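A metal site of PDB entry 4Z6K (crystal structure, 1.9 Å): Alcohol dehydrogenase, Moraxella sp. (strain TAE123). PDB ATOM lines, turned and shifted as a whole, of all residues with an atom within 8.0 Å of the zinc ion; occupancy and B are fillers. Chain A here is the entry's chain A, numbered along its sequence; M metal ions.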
ATOM      1  N   GLY A  36     -12.705 -15.978  12.498  1.00  0.00           N
ATOM      2  CA  GLY A  36     -11.272 -15.916  12.548  1.00  0.00           C
ATOM      3  C   GLY A  36     -10.636 -17.001  11.693  1.00  0.00           C
ATOM      4  O   GLY A  36     -11.248 -18.000  11.374  1.00  0.00           O
ATOM      5  N   VAL A  37      -9.409 -16.774  11.280  1.00  0.00           N
ATOM      6  CA  VAL A  37      -8.548 -17.799  10.683  1.00  0.00           C
ATOM      7  C   VAL A  37      -7.256 -17.953  11.470  1.00  0.00           C
ATOM      8  O   VAL A  37      -6.724 -16.954  11.952  1.00  0.00           O
ATOM      9  CB  VAL A  37      -8.114 -17.260   9.309  1.00  0.00           C
ATOM     10  CG1 VAL A  37      -7.375 -18.306   8.505  1.00  0.00           C
ATOM     11  CG2 VAL A  37      -9.337 -16.779   8.559  1.00  0.00           C
ATOM     12  N   CYS A  38      -6.736 -19.165  11.600  1.00  0.00           N
ATOM     13  CA  CYS A  38      -5.438 -19.324  12.319  1.00  0.00           C
ATOM     14  C   CYS A  38      -4.649 -20.503  11.795  1.00  0.00           C
ATOM     15  O   CYS A  38      -5.151 -21.215  10.908  1.00  0.00           O
ATOM     16  CB  CYS A  38      -5.630 -19.471  13.857  1.00  0.00           C
ATOM     17  SG  CYS A  38      -6.029 -21.089  14.467  1.00  0.00           S
ATOM     18  N   HIS A  39      -3.460 -20.740  12.363  1.00  0.00           N
ATOM     19  CA  HIS A  39      -2.630 -21.843  11.909  1.00  0.00           C
ATOM     20  C   HIS A  39      -3.349 -23.219  12.077  1.00  0.00           C
ATOM     21  O   HIS A  39      -3.001 -24.166  11.389  1.00  0.00           O
ATOM     22  CB  HIS A  39      -1.324 -21.920  12.704  1.00  0.00           C
ATOM     23  CG  HIS A  39      -0.362 -20.894  12.331  1.00  0.00           C
ATOM     24  ND1 HIS A  39       0.549 -21.051  11.302  1.00  0.00           N
ATOM     25  CD2 HIS A  39      -0.195 -19.638  12.799  1.00  0.00           C
ATOM     26  CE1 HIS A  39       1.230 -19.934  11.150  1.00  0.00           C
ATOM     27  NE2 HIS A  39       0.798 -19.065  12.043  1.00  0.00           N
ATOM     28  N   THR A  40      -4.288 -23.334  12.975  1.00  0.00           N
ATOM     29  CA  THR A  40      -4.952 -24.618  13.177  1.00  0.00           C
ATOM     30  C   THR A  40      -5.760 -24.954  11.947  1.00  0.00           C
ATOM     31  O   THR A  40      -5.825 -26.093  11.520  1.00  0.00           O
ATOM     32  CB  THR A  40      -5.841 -24.575  14.406  1.00  0.00           C
ATOM     33  OG1 THR A  40      -5.033 -24.685  15.547  1.00  0.00           O
ATOM     34  CG2 THR A  40      -6.777 -25.729  14.448  1.00  0.00           C
ATOM     35  N   ASP A  41      -6.381 -23.956  11.347  1.00  0.00           N
ATOM     36  CA  ASP A  41      -7.074 -24.153  10.076  1.00  0.00           C
ATOM     37  C   ASP A  41      -6.108 -24.563   8.975  1.00  0.00           C
ATOM     38  O   ASP A  41      -6.450 -25.324   8.096  1.00  0.00           O
ATOM     39  CB  ASP A  41      -7.766 -22.843   9.640  1.00  0.00           C
ATOM     40  CG  ASP A  41      -8.880 -22.413  10.618  1.00  0.00           C
ATOM     41  OD1 ASP A  41      -8.823 -21.268  11.133  1.00  0.00           O
ATOM     42  OD2 ASP A  41      -9.816 -23.187  10.876  1.00  0.00           O
ATOM     43  N   GLY A  60     -12.736 -23.728  10.033  1.00  0.00           N
ATOM     44  CA  GLY A  60     -13.069 -22.494  10.755  1.00  0.00           C
ATOM     45  C   GLY A  60     -13.629 -22.870  12.147  1.00  0.00           C
ATOM     46  O   GLY A  60     -14.568 -23.611  12.213  1.00  0.00           O
ATOM     47  N   HIS A  61     -13.021 -22.340  13.233  1.00  0.00           N
ATOM     48  CA  HIS A  61     -13.435 -22.597  14.575  1.00  0.00           C
ATOM     49  C   HIS A  61     -13.392 -21.311  15.371  1.00  0.00           C
ATOM     50  O   HIS A  61     -13.145 -21.343  16.556  1.00  0.00           O
ATOM     51  CB  HIS A  61     -12.532 -23.646  15.284  1.00  0.00           C
ATOM     52  CG  HIS A  61     -11.086 -23.347  15.151  1.00  0.00           C
ATOM     53  ND1 HIS A  61     -10.365 -23.730  14.050  1.00  0.00           N
ATOM     54  CD2 HIS A  61     -10.275 -22.513  15.859  1.00  0.00           C
ATOM     55  CE1 HIS A  61      -9.142 -23.219  14.120  1.00  0.00           C
ATOM     56  NE2 HIS A  61      -9.084 -22.420  15.174  1.00  0.00           N
ATOM     57  N   GLU A  62     -13.749 -20.185  14.740  1.00  0.00           N
ATOM     58  CA  GLU A  62     -13.773 -18.879  15.434  1.00  0.00           C
ATOM     59  C   GLU A  62     -14.893 -18.008  14.795  1.00  0.00           C
ATOM     60  O   GLU A  62     -14.631 -16.973  14.229  1.00  0.00           O
ATOM     61  CB  GLU A  62     -12.526 -18.064  15.259  1.00  0.00           C
ATOM     62  CG  GLU A  62     -11.332 -18.452  15.964  1.00  0.00           C
ATOM     63  CD  GLU A  62     -10.122 -17.699  15.448  1.00  0.00           C
ATOM     64  OE1 GLU A  62      -9.196 -18.418  14.997  1.00  0.00           O
ATOM     65  OE2 GLU A  62     -10.139 -16.448  15.459  1.00  0.00           O
ATOM     66  N   TRP A  87     -13.531 -23.976  18.930  1.00  0.00           N
ATOM     67  CA  TRP A  87     -12.875 -25.217  18.588  1.00  0.00           C
ATOM     68  C   TRP A  87     -13.618 -26.393  19.202  1.00  0.00           C
ATOM     69  O   TRP A  87     -13.834 -27.392  18.523  1.00  0.00           O
ATOM     70  CB  TRP A  87     -11.471 -25.227  19.126  1.00  0.00           C
ATOM     71  CG  TRP A  87     -10.729 -26.528  19.039  1.00  0.00           C
ATOM     72  CD1 TRP A  87     -10.398 -27.344  20.077  1.00  0.00           C
ATOM     73  CD2 TRP A  87     -10.170 -27.146  17.855  1.00  0.00           C
ATOM     74  NE1 TRP A  87      -9.637 -28.394  19.618  1.00  0.00           N
ATOM     75  CE2 TRP A  87      -9.488 -28.315  18.275  1.00  0.00           C
ATOM     76  CE3 TRP A  87     -10.210 -26.851  16.493  1.00  0.00           C
ATOM     77  CZ2 TRP A  87      -8.860 -29.170  17.375  1.00  0.00           C
ATOM     78  CZ3 TRP A  87      -9.623 -27.716  15.604  1.00  0.00           C
ATOM     79  CH2 TRP A  87      -8.901 -28.838  16.042  1.00  0.00           C
ATOM     80  N   ALA A 144     -13.937 -11.974  17.557  1.00  0.00           N
ATOM     81  CA  ALA A 144     -13.793 -13.308  17.037  1.00  0.00           C
ATOM     82  C   ALA A 144     -12.504 -14.037  17.528  1.00  0.00           C
ATOM     83  O   ALA A 144     -12.573 -15.209  17.887  1.00  0.00           O
ATOM     84  CB  ALA A 144     -13.836 -13.321  15.517  1.00  0.00           C
ATOM     85  N   PRO A 145     -11.338 -13.391  17.453  1.00  0.00           N
ATOM     86  CA  PRO A 145     -10.133 -14.056  17.909  1.00  0.00           C
ATOM     87  C   PRO A 145     -10.112 -14.494  19.396  1.00  0.00           C
ATOM     88  O   PRO A 145      -9.332 -15.343  19.752  1.00  0.00           O
ATOM     89  CB  PRO A 145      -9.046 -13.043  17.624  1.00  0.00           C
ATOM     90  CG  PRO A 145      -9.608 -12.196  16.455  1.00  0.00           C
ATOM     91  CD  PRO A 145     -11.022 -12.044  16.959  1.00  0.00           C
ATOM     92  N   LEU A 147     -12.346 -16.176  20.705  1.00  0.00           N
ATOM     93  CA  LEU A 147     -12.800 -17.555  20.694  1.00  0.00           C
ATOM     94  C   LEU A 147     -11.730 -18.654  20.531  1.00  0.00           C
ATOM     95  O   LEU A 147     -11.967 -19.786  20.840  1.00  0.00           O
ATOM     96  CB  LEU A 147     -13.846 -17.750  19.613  1.00  0.00           C
ATOM     97  CG  LEU A 147     -15.037 -16.775  19.585  1.00  0.00           C
ATOM     98  CD1 LEU A 147     -15.829 -16.985  18.270  1.00  0.00           C
ATOM     99  CD2 LEU A 147     -15.904 -16.954  20.764  1.00  0.00           C
ATOM    100  N   CYS A 148     -10.570 -18.279  20.038  1.00  0.00           N
ATOM    101  CA  CYS A 148      -9.533 -19.215  19.851  1.00  0.00           C
ATOM    102  C   CYS A 148      -8.276 -18.680  20.530  1.00  0.00           C
ATOM    103  O   CYS A 148      -7.749 -19.287  21.481  1.00  0.00           O
ATOM    104  CB  CYS A 148      -9.270 -19.424  18.359  1.00  0.00           C
ATOM    105  SG  CYS A 148      -7.692 -20.255  17.942  1.00  0.00           S
ATOM    106  N   ALA A 149      -7.662 -17.637  19.972  1.00  0.00           N
ATOM    107  CA  ALA A 149      -6.434 -17.117  20.564  1.00  0.00           C
ATOM    108  C   ALA A 149      -6.602 -16.698  22.040  1.00  0.00           C
ATOM    109  O   ALA A 149      -5.759 -16.976  22.873  1.00  0.00           O
ATOM    110  CB  ALA A 149      -5.891 -15.945  19.784  1.00  0.00           C
ATOM    111  N   THR A 152      -7.293 -19.632  24.530  1.00  0.00           N
ATOM    112  CA  THR A 152      -6.107 -20.432  24.608  1.00  0.00           C
ATOM    113  C   THR A 152      -5.068 -19.818  25.505  1.00  0.00           C
ATOM    114  O   THR A 152      -4.512 -20.525  26.339  1.00  0.00           O
ATOM    115  CB  THR A 152      -5.529 -20.564  23.196  1.00  0.00           C
ATOM    116  OG1 THR A 152      -6.370 -21.406  22.459  1.00  0.00           O
ATOM    117  CG2 THR A 152      -4.195 -21.119  23.224  1.00  0.00           C
ATOM    118  N   LEU A 176      -1.114 -15.193  18.965  1.00  0.00           N
ATOM    119  CA  LEU A 176      -1.383 -15.477  20.380  1.00  0.00           C
ATOM    120  C   LEU A 176      -0.742 -14.537  21.394  1.00  0.00           C
ATOM    121  O   LEU A 176      -1.377 -14.191  22.375  1.00  0.00           O
ATOM    122  CB  LEU A 176      -0.899 -16.891  20.697  1.00  0.00           C
ATOM    123  CG  LEU A 176      -1.627 -18.055  20.011  1.00  0.00           C
ATOM    124  CD1 LEU A 176      -1.044 -19.322  20.637  1.00  0.00           C
ATOM    125  CD2 LEU A 176      -3.119 -18.076  20.282  1.00  0.00           C
ATOM    126  N   ARG A 331      -4.248 -10.974  13.974  1.00  0.00           N
ATOM    127  CA  ARG A 331      -5.053 -12.053  13.491  1.00  0.00           C
ATOM    128  C   ARG A 331      -5.833 -11.584  12.254  1.00  0.00           C
ATOM    129  O   ARG A 331      -6.164 -10.428  12.136  1.00  0.00           O
ATOM    130  CB  ARG A 331      -6.001 -12.468  14.586  1.00  0.00           C
ATOM    131  CG  ARG A 331      -5.276 -13.069  15.828  1.00  0.00           C
ATOM    132  CD  ARG A 331      -4.829 -14.490  15.607  1.00  0.00           C
ATOM    133  NE  ARG A 331      -5.975 -15.356  15.759  1.00  0.00           N
ATOM    134  CZ  ARG A 331      -5.858 -16.608  16.135  1.00  0.00           C
ATOM    135  NH1 ARG A 331      -6.907 -17.327  16.307  1.00  0.00           N
ATOM    136  NH2 ARG A 331      -4.651 -17.096  16.335  1.00  0.00           N
HETATM  137 ZN    ZN M   1      -7.910 -20.617  15.636  1.00  0.00          ZN
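The side-chain carboxylate of Asp 41 sits at hydrogen-bond distance from a ring nitrogen (ND1) of His 61 (3.3 Å). SG of Cys 38 sits close to N of Thr 40, at 3.2 Å. The side-chain carboxylate (OD1) of Asp 41 is in hydrogen-bond range of the backbone NH (N) of Cys 38, at 3.0 Å. SG of Cys 148 sits close to OE1 of Glu 62. The guanidinium group (NH1) of Arg 331 lies close to the side-chain sulfur (SG) of Cys 148 (3.4 Å). O of Cys 148 sits at hydrogen-bond distance from OG1 of Thr 152 (2.7 Å). The side-chain carboxylate (OE1) of Glu 62 is in salt-bridge range of the guanidinium group (NH1) of Arg 331. O of Glu 62 is in hydrogen-bond range of N of Gly 36 (2.8 Å).
Arg 331 touches the zinc ion. Within 4 Å of the zinc ion: Cys 38, His 61, Glu 62, Cys 148 and Arg 331.
The zinc ion is bound by NE2 of His 61 (2.2 Å), SG of Cys 38 (2.3 Å) and SG of Cys 148 (2.3 Å). The zinc ion has three donor atoms within binding distance. Slightly farther from the zinc ion lies OE1 of Glu 62 (2.6 Å).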
